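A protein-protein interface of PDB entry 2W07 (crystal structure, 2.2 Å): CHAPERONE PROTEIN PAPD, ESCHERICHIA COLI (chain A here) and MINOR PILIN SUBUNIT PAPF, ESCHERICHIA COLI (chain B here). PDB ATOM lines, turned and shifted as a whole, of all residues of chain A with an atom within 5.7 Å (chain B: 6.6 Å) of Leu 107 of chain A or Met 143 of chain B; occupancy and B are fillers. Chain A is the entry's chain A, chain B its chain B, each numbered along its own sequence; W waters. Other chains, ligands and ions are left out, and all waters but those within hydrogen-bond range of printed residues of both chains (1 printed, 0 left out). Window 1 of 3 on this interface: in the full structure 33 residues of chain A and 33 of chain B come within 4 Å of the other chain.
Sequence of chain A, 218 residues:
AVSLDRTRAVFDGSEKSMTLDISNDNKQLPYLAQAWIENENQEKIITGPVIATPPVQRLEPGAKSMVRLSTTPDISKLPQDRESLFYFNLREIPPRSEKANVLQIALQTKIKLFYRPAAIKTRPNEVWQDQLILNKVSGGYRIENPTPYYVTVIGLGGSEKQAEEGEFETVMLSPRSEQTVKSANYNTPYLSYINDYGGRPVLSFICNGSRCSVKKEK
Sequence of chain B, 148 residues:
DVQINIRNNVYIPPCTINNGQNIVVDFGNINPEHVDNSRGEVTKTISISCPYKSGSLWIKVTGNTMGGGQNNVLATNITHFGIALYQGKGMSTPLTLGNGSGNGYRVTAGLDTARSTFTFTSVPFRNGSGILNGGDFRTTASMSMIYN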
ATOM      1  N   ALA A   1      18.866  17.799  20.019  1.00  0.00           N
ATOM      2  CA  ALA A   1      19.824  16.760  19.556  1.00  0.00           C
ATOM      3  C   ALA A   1      21.047  16.670  20.457  1.00  0.00           C
ATOM      4  O   ALA A   1      21.513  17.668  21.014  1.00  0.00           O
ATOM      5  CB  ALA A   1      20.254  17.039  18.120  1.00  0.00           C
ATOM      6  N   LEU A  90      27.568   8.006  17.929  1.00  0.00           N
ATOM      7  CA  LEU A  90      26.616   8.424  18.947  1.00  0.00           C
ATOM      8  C   LEU A  90      25.281   8.685  18.268  1.00  0.00           C
ATOM      9  O   LEU A  90      25.155   9.605  17.463  1.00  0.00           O
ATOM     10  CB  LEU A  90      27.082   9.700  19.653  1.00  0.00           C
ATOM     11  CG  LEU A  90      26.184  10.110  20.828  1.00  0.00           C
ATOM     12  CD1 LEU A  90      26.336   9.106  21.963  1.00  0.00           C
ATOM     13  CD2 LEU A  90      26.562  11.495  21.310  1.00  0.00           C
ATOM     14  N   ARG A  91      24.288   7.862  18.574  1.00  0.00           N
ATOM     15  CA  ARG A  91      22.968   8.042  17.993  1.00  0.00           C
ATOM     16  C   ARG A  91      21.954   8.371  19.084  1.00  0.00           C
ATOM     17  O   ARG A  91      21.915   7.732  20.132  1.00  0.00           O
ATOM     18  CB  ARG A  91      22.522   6.788  17.246  1.00  0.00           C
ATOM     19  CG  ARG A  91      21.148   6.935  16.599  1.00  0.00           C
ATOM     20  CD  ARG A  91      20.927   5.876  15.541  1.00  0.00           C
ATOM     21  NE  ARG A  91      20.791   4.547  16.117  1.00  0.00           N
ATOM     22  CZ  ARG A  91      20.874   3.419  15.416  1.00  0.00           C
ATOM     23  NH1 ARG A  91      20.729   2.246  16.025  1.00  0.00           N
ATOM     24  NH2 ARG A  91      21.119   3.460  14.112  1.00  0.00           N
ATOM     25  N   GLU A  92      21.132   9.373  18.822  1.00  0.00           N
ATOM     26  CA  GLU A  92      20.132   9.787  19.789  1.00  0.00           C
ATOM     27  C   GLU A  92      18.807   9.078  19.562  1.00  0.00           C
ATOM     28  O   GLU A  92      18.391   8.857  18.424  1.00  0.00           O
ATOM     29  CB  GLU A  92      19.928  11.296  19.697  1.00  0.00           C
ATOM     30  CG  GLU A  92      19.646  11.762  18.291  1.00  0.00           C
ATOM     31  CD  GLU A  92      19.375  13.242  18.205  1.00  0.00           C
ATOM     32  OE1 GLU A  92      20.207  14.024  18.698  1.00  0.00           O
ATOM     33  OE2 GLU A  92      18.329  13.619  17.637  1.00  0.00           O
ATOM     34  N   PRO A  94      15.185   9.785  20.181  1.00  0.00           N
ATOM     35  CA  PRO A  94      14.222  10.822  20.554  1.00  0.00           C
ATOM     36  C   PRO A  94      12.987  10.281  21.254  1.00  0.00           C
ATOM     37  O   PRO A  94      12.679   9.094  21.170  1.00  0.00           O
ATOM     38  CB  PRO A  94      13.895  11.478  19.214  1.00  0.00           C
ATOM     39  CG  PRO A  94      13.963  10.325  18.268  1.00  0.00           C
ATOM     40  CD  PRO A  94      15.218   9.603  18.718  1.00  0.00           C
ATOM     41  N   ILE A 105      12.998  11.328  12.888  1.00  0.00           N
ATOM     42  CA  ILE A 105      14.397  11.232  12.507  1.00  0.00           C
ATOM     43  C   ILE A 105      15.265  11.095  13.752  1.00  0.00           C
ATOM     44  O   ILE A 105      15.159  11.886  14.691  1.00  0.00           O
ATOM     45  CB  ILE A 105      14.858  12.480  11.725  1.00  0.00           C
ATOM     46  CG1 ILE A 105      14.085  12.595  10.404  1.00  0.00           C
ATOM     47  CG2 ILE A 105      16.353  12.411  11.475  1.00  0.00           C
ATOM     48  CD1 ILE A 105      14.191  11.381   9.501  1.00  0.00           C
ATOM     49  N   ALA A 106      16.109  10.072  13.763  1.00  0.00           N
ATOM     50  CA  ALA A 106      17.019   9.853  14.877  1.00  0.00           C
ATOM     51  C   ALA A 106      18.385  10.303  14.378  1.00  0.00           C
ATOM     52  O   ALA A 106      18.956   9.693  13.470  1.00  0.00           O
ATOM     53  CB  ALA A 106      17.053   8.378  15.254  1.00  0.00           C
ATOM     54  N   LEU A 107      18.897  11.386  14.950  1.00  0.00           N
ATOM     55  CA  LEU A 107      20.192  11.898  14.544  1.00  0.00           C
ATOM     56  C   LEU A 107      21.354  11.073  15.100  1.00  0.00           C
ATOM     57  O   LEU A 107      21.300  10.560  16.218  1.00  0.00           O
ATOM     58  CB  LEU A 107      20.335  13.361  14.964  1.00  0.00           C
ATOM     59  CG  LEU A 107      19.451  14.344  14.185  1.00  0.00           C
ATOM     60  CD1 LEU A 107      19.681  15.766  14.704  1.00  0.00           C
ATOM     61  CD2 LEU A 107      19.781  14.263  12.689  1.00  0.00           C
ATOM     62  N   GLN A 108      22.401  10.951  14.299  1.00  0.00           N
ATOM     63  CA  GLN A 108      23.592  10.201  14.681  1.00  0.00           C
ATOM     64  C   GLN A 108      24.835  10.946  14.223  1.00  0.00           C
ATOM     65  O   GLN A 108      24.833  11.587  13.174  1.00  0.00           O
ATOM     66  CB  GLN A 108      23.581   8.818  14.020  1.00  0.00           C
ATOM     67  CG  GLN A 108      24.762   7.923  14.381  1.00  0.00           C
ATOM     68  CD  GLN A 108      24.717   6.591  13.652  1.00  0.00           C
ATOM     69  OE1 GLN A 108      23.664   5.951  13.575  1.00  0.00           O
ATOM     70  NE2 GLN A 108      25.859   6.163  13.115  1.00  0.00           N
ATOM     71  N   THR A 109      25.887  10.872  15.026  1.00  0.00           N
ATOM     72  CA  THR A 109      27.155  11.494  14.677  1.00  0.00           C
ATOM     73  C   THR A 109      28.196  10.387  14.564  1.00  0.00           C
ATOM     74  O   THR A 109      28.264   9.488  15.412  1.00  0.00           O
ATOM     75  CB  THR A 109      27.624  12.496  15.751  1.00  0.00           C
ATOM     76  OG1 THR A 109      26.580  13.441  16.016  1.00  0.00           O
ATOM     77  CG2 THR A 109      28.854  13.235  15.269  1.00  0.00           C
ATOM     78  N   ILE B  17      22.504  20.606  14.432  1.00  0.00           N
ATOM     79  CA  ILE B  17      21.452  20.295  13.472  1.00  0.00           C
ATOM     80  C   ILE B  17      20.109  20.901  13.852  1.00  0.00           C
ATOM     81  O   ILE B  17      19.529  20.571  14.891  1.00  0.00           O
ATOM     82  CB  ILE B  17      21.313  18.772  13.304  1.00  0.00           C
ATOM     83  CG1 ILE B  17      22.687  18.169  12.990  1.00  0.00           C
ATOM     84  CG2 ILE B  17      20.332  18.458  12.191  1.00  0.00           C
ATOM     85  CD1 ILE B  17      23.390  18.802  11.792  1.00  0.00           C
ATOM     86  N   ASN B  18      19.629  21.775  12.967  1.00  0.00           N
ATOM     87  CA  ASN B  18      18.390  22.525  13.130  1.00  0.00           C
ATOM     88  C   ASN B  18      18.157  22.941  14.586  1.00  0.00           C
ATOM     89  O   ASN B  18      17.147  22.623  15.211  1.00  0.00           O
ATOM     90  CB  ASN B  18      17.198  21.759  12.526  1.00  0.00           C
ATOM     91  CG  ASN B  18      16.540  20.822  13.495  1.00  0.00           C
ATOM     92  OD1 ASN B  18      17.203  20.019  14.145  1.00  0.00           O
ATOM     93  ND2 ASN B  18      15.211  20.907  13.590  1.00  0.00           N
ATOM     94  N   GLY B  20      19.414  22.041  17.524  1.00  0.00           N
ATOM     95  CA  GLY B  20      19.188  21.033  18.544  1.00  0.00           C
ATOM     96  C   GLY B  20      17.743  20.648  18.796  1.00  0.00           C
ATOM     97  O   GLY B  20      17.437  20.041  19.825  1.00  0.00           O
ATOM     98  N   GLN B  21      16.856  20.992  17.865  1.00  0.00           N
ATOM     99  CA  GLN B  21      15.445  20.661  18.009  1.00  0.00           C
ATOM    100  C   GLN B  21      15.181  19.273  17.445  1.00  0.00           C
ATOM    101  O   GLN B  21      15.985  18.735  16.692  1.00  0.00           O
ATOM    102  CB  GLN B  21      14.584  21.692  17.288  1.00  0.00           C
ATOM    103  N   ILE B  23      13.503  16.431  15.107  1.00  0.00           N
ATOM    104  CA  ILE B  23      13.065  16.401  13.717  1.00  0.00           C
ATOM    105  C   ILE B  23      11.979  15.361  13.514  1.00  0.00           C
ATOM    106  O   ILE B  23      12.197  14.165  13.711  1.00  0.00           O
ATOM    107  CB  ILE B  23      14.236  16.081  12.767  1.00  0.00           C
ATOM    108  CG1 ILE B  23      15.300  17.172  12.872  1.00  0.00           C
ATOM    109  CG2 ILE B  23      13.732  15.959  11.329  1.00  0.00           C
ATOM    110  CD1 ILE B  23      16.526  16.905  12.033  1.00  0.00           C
ATOM    111  N   ILE B  46      16.175  20.839   7.042  1.00  0.00           N
ATOM    112  CA  ILE B  46      16.850  20.947   8.323  1.00  0.00           C
ATOM    113  C   ILE B  46      18.177  21.683   8.146  1.00  0.00           C
ATOM    114  O   ILE B  46      18.966  21.367   7.255  1.00  0.00           O
ATOM    115  CB  ILE B  46      17.064  19.550   8.947  1.00  0.00           C
ATOM    116  CG1 ILE B  46      17.927  18.679   8.039  1.00  0.00           C
ATOM    117  CG2 ILE B  46      15.718  18.867   9.144  1.00  0.00           C
ATOM    118  CD1 ILE B  46      19.395  18.758   8.340  1.00  0.00           C
ATOM    119  N   ILE B  59      26.039  12.635   4.772  1.00  0.00           N
ATOM    120  CA  ILE B  59      24.792  12.227   5.397  1.00  0.00           C
ATOM    121  C   ILE B  59      24.270  10.920   4.824  1.00  0.00           C
ATOM    122  O   ILE B  59      24.032  10.811   3.617  1.00  0.00           O
ATOM    123  CB  ILE B  59      23.688  13.280   5.228  1.00  0.00           C
ATOM    124  CG1 ILE B  59      24.066  14.563   5.964  1.00  0.00           C
ATOM    125  CG2 ILE B  59      22.371  12.730   5.760  1.00  0.00           C
ATOM    126  CD1 ILE B  59      22.976  15.619   5.940  1.00  0.00           C
ATOM    127  N   LYS B  60      24.092   9.937   5.700  1.00  0.00           N
ATOM    128  CA  LYS B  60      23.570   8.639   5.305  1.00  0.00           C
ATOM    129  C   LYS B  60      22.298   8.379   6.101  1.00  0.00           C
ATOM    130  O   LYS B  60      22.240   8.637   7.303  1.00  0.00           O
ATOM    131  CB  LYS B  60      24.600   7.543   5.576  1.00  0.00           C
ATOM    132  N   VAL B  61      21.275   7.878   5.422  1.00  0.00           N
ATOM    133  CA  VAL B  61      20.000   7.590   6.061  1.00  0.00           C
ATOM    134  C   VAL B  61      19.742   6.091   6.033  1.00  0.00           C
ATOM    135  O   VAL B  61      19.812   5.463   4.971  1.00  0.00           O
ATOM    136  CB  VAL B  61      18.848   8.295   5.327  1.00  0.00           C
ATOM    137  CG1 VAL B  61      17.531   8.014   6.041  1.00  0.00           C
ATOM    138  CG2 VAL B  61      19.125   9.794   5.244  1.00  0.00           C
ATOM    139  N   THR B  62      19.436   5.520   7.193  1.00  0.00           N
ATOM    140  CA  THR B  62      19.172   4.092   7.272  1.00  0.00           C
ATOM    141  C   THR B  62      17.952   3.778   8.139  1.00  0.00           C
ATOM    142  O   THR B  62      17.455   4.633   8.872  1.00  0.00           O
ATOM    143  CB  THR B  62      20.399   3.337   7.829  1.00  0.00           C
ATOM    144  OG1 THR B  62      20.666   3.780   9.165  1.00  0.00           O
ATOM    145  CG2 THR B  62      21.628   3.614   6.967  1.00  0.00           C
ATOM    146  N   LEU B  95      16.157   8.990  -2.582  1.00  0.00           N
ATOM    147  CA  LEU B  95      17.140   9.051  -1.506  1.00  0.00           C
ATOM    148  C   LEU B  95      17.391   7.651  -0.961  1.00  0.00           C
ATOM    149  O   LEU B  95      16.712   7.204  -0.040  1.00  0.00           O
ATOM    150  CB  LEU B  95      16.644   9.963  -0.381  1.00  0.00           C
ATOM    151  CG  LEU B  95      17.485  10.001   0.898  1.00  0.00           C
ATOM    152  CD1 LEU B  95      18.932  10.326   0.569  1.00  0.00           C
ATOM    153  CD2 LEU B  95      16.907  11.037   1.846  1.00  0.00           C
ATOM    154  N   PHE B 118      19.780  20.888   4.446  1.00  0.00           N
ATOM    155  CA  PHE B 118      19.540  19.599   3.817  1.00  0.00           C
ATOM    156  C   PHE B 118      18.029  19.431   3.720  1.00  0.00           C
ATOM    157  O   PHE B 118      17.318  19.479   4.729  1.00  0.00           O
ATOM    158  CB  PHE B 118      20.137  18.458   4.644  1.00  0.00           C
ATOM    159  CG  PHE B 118      19.958  17.100   4.019  1.00  0.00           C
ATOM    160  CD1 PHE B 118      20.571  16.789   2.808  1.00  0.00           C
ATOM    161  CD2 PHE B 118      19.170  16.132   4.637  1.00  0.00           C
ATOM    162  CE1 PHE B 118      20.405  15.534   2.220  1.00  0.00           C
ATOM    163  CE2 PHE B 118      18.997  14.868   4.056  1.00  0.00           C
ATOM    164  CZ  PHE B 118      19.615  14.571   2.844  1.00  0.00           C
ATOM    165  N   PHE B 120      14.805  17.055   2.258  1.00  0.00           N
ATOM    166  CA  PHE B 120      14.422  15.726   1.803  1.00  0.00           C
ATOM    167  C   PHE B 120      12.910  15.618   1.789  1.00  0.00           C
ATOM    168  O   PHE B 120      12.224  16.217   2.617  1.00  0.00           O
ATOM    169  CB  PHE B 120      15.045  14.632   2.685  1.00  0.00           C
ATOM    170  CG  PHE B 120      14.514  14.585   4.090  1.00  0.00           C
ATOM    171  CD1 PHE B 120      13.607  13.601   4.470  1.00  0.00           C
ATOM    172  CD2 PHE B 120      14.948  15.500   5.046  1.00  0.00           C
ATOM    173  CE1 PHE B 120      13.140  13.522   5.784  1.00  0.00           C
ATOM    174  CE2 PHE B 120      14.489  15.434   6.362  1.00  0.00           C
ATOM    175  CZ  PHE B 120      13.582  14.440   6.731  1.00  0.00           C
ATOM    176  N   ALA B 141      13.801   6.681  11.165  1.00  0.00           N
ATOM    177  CA  ALA B 141      14.967   6.538  10.308  1.00  0.00           C
ATOM    178  C   ALA B 141      16.150   7.207  11.004  1.00  0.00           C
ATOM    179  O   ALA B 141      15.975   8.161  11.761  1.00  0.00           O
ATOM    180  CB  ALA B 141      14.712   7.204   8.957  1.00  0.00           C
ATOM    181  N   SER B 142      17.350   6.698  10.756  1.00  0.00           N
ATOM    182  CA  SER B 142      18.538   7.282  11.357  1.00  0.00           C
ATOM    183  C   SER B 142      19.201   8.176  10.322  1.00  0.00           C
ATOM    184  O   SER B 142      19.309   7.814   9.158  1.00  0.00           O
ATOM    185  CB  SER B 142      19.516   6.195  11.797  1.00  0.00           C
ATOM    186  OG  SER B 142      18.899   5.295  12.697  1.00  0.00           O
ATOM    187  N   MET B 143      19.619   9.357  10.749  1.00  0.00           N
ATOM    188  CA  MET B 143      20.293  10.280   9.859  1.00  0.00           C
ATOM    189  C   MET B 143      21.670  10.524  10.461  1.00  0.00           C
ATOM    190  O   MET B 143      21.801  11.224  11.470  1.00  0.00           O
ATOM    191  CB  MET B 143      19.501  11.583   9.747  1.00  0.00           C
ATOM    192  CG  MET B 143      20.134  12.616   8.848  1.00  0.00           C
ATOM    193  SD  MET B 143      19.024  14.003   8.558  1.00  0.00           S
ATOM    194  CE  MET B 143      18.038  13.337   7.190  1.00  0.00           C
ATOM    195  N   SER B 144      22.689   9.928   9.844  1.00  0.00           N
ATOM    196  CA  SER B 144      24.060  10.045  10.324  1.00  0.00           C
ATOM    197  C   SER B 144      24.884  11.146   9.684  1.00  0.00           C
ATOM    198  O   SER B 144      24.982  11.243   8.458  1.00  0.00           O
ATOM    199  CB  SER B 144      24.808   8.722  10.134  1.00  0.00           C
ATOM    200  OG  SER B 144      24.197   7.678  10.864  1.00  0.00           O
ATOM    201  N   MET B 145      25.476  11.974  10.533  1.00  0.00           N
ATOM    202  CA  MET B 145      26.349  13.043  10.078  1.00  0.00           C
ATOM    203  C   MET B 145      27.734  12.419  10.228  1.00  0.00           C
ATOM    204  O   MET B 145      28.210  12.188  11.340  1.00  0.00           O
ATOM    205  CB  MET B 145      26.209  14.277  10.980  1.00  0.00           C
ATOM    206  CG  MET B 145      25.295  15.371  10.426  1.00  0.00           C
ATOM    207  SD  MET B 145      23.707  14.784   9.795  1.00  0.00           S
ATOM    208  CE  MET B 145      23.048  14.018  11.268  1.00  0.00           C
HETATM  209  O   HOH W   1      15.450  14.294  15.821  1.00  0.00           O
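The side-chain hydroxyl (OG) of Ser 142 of chain B lies within hydrogen-bond range of the guanidinium group (NH2) of Arg 91 of chain A.
The backbone NH (N) of Gln 108 of chain A sits at hydrogen-bond distance from the backbone carbonyl oxygen (O) of Met 143 of chain B.
NE2 of Gln 108 of chain A sits close to OG of Ser 144 of chain B, at 3.2 Å.
N of Met 143 of chain B sits at hydrogen-bond distance from O of Ala 106 of chain A (2.8 Å).
The backbone NH (N) of Ala 106 of chain A is in hydrogen-bond range of the backbone carbonyl oxygen (O) of Ala 141 of chain B (2.8 Å).
N of Ala 1 of chain A is in hydrogen-bond range of O of Gly 20 of chain B (2.7 Å).
The backbone NH (N) of Ile 105 of chain A lies within hydrogen-bond range of the backbone carbonyl oxygen (O) of Ile 23 of chain B.
The backbone carbonyl oxygen (O) of Gln 108 of chain A sits at hydrogen-bond distance from the backbone NH (N) of Met 145 of chain B (2.7 Å).
O of Leu 90 of chain A lies within hydrogen-bond range of N of Thr 109 of chain A (2.8 Å).
The backbone NH of Ser 144 of chain B sits at hydrogen-bond distance from the backbone carbonyl oxygen of Lys 60 of chain B (2.9 Å).
O of Thr 62 of chain B sits at hydrogen-bond distance from N of Ser 142 of chain B (2.8 Å).
The backbone NH (N) of Glu 92 of chain A sits at hydrogen-bond distance from the backbone carbonyl oxygen (O) of Leu 107 of chain A (2.9 Å).
Among the printed residues, merely in contact across the chains: Ala 106 of chain A with Ser 142 of chain B (3.2 Å), Ile 105 of chain A with Ala 141 of chain B (3.5 Å), Leu 107 of chain A with Met 143 of chain B (3.5 Å), Thr 109 of chain A with Met 145 of chain B (3.6 Å), Leu 107 of chain A with Met 145 of chain B (3.6 Å), Ile 105 of chain A with Met 143 of chain B (3.7 Å) and Leu 107 of chain A with Ile 17 of chain B (3.7 Å).
Of chain B, only Ile 17, Met 143 and Met 145 come within 4 Å of Leu 107 of chain A.
Met 143 of chain B touches just these residues of chain A: Ile 105 (3.7 Å), Ala 106 (2.8 Å), Leu 107 (3.5 Å) and Gln 108 (2.9 Å).
Printed residues of chain B within 4 Å of Thr 109 of chain A: Met 145.
Of the printed residues of chain B, Ala 1 of chain A touches Gly 20.
Of the printed residues of chain A, Ala 141 of chain B touches Ile 105 and Ala 106.
Of the printed residues of chain B, Gln 108 of chain A touches Met 143 (2.9 Å), Ser 144 (3.0 Å) and Met 145 (2.7 Å).
Ile 46 of chain B touches none of the printed residues of chain A.
The nearest printed residue of chain B that does not touch Arg 91 of chain A is Thr 62 of chain B (5.0 Å).
Of the 10 printed residues of chain A, 7 touch a printed residue of chain B.
Hydrophobic or aromatic side chains of chain A within 4 Å of the printed part of chain B: Ile 105, Ala 106 and Leu 107.
Of the 18 printed residues of chain B, 8 touch a printed residue of chain A.
Hydrophobic or aromatic side chains of chain B within 4 Å of the printed part of chain A: Ile 17, Ile 23, Met 143 and Met 145.
Among the printed residues, 15 pairs touch across the chains.
Water W1 lies within hydrogen-bond range of O of Ile 105 of chain A (2.7 Å), N of Ile 23 of chain B (3.0 Å) and OE2 of Glu 92 of chain A (3.5 Å).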
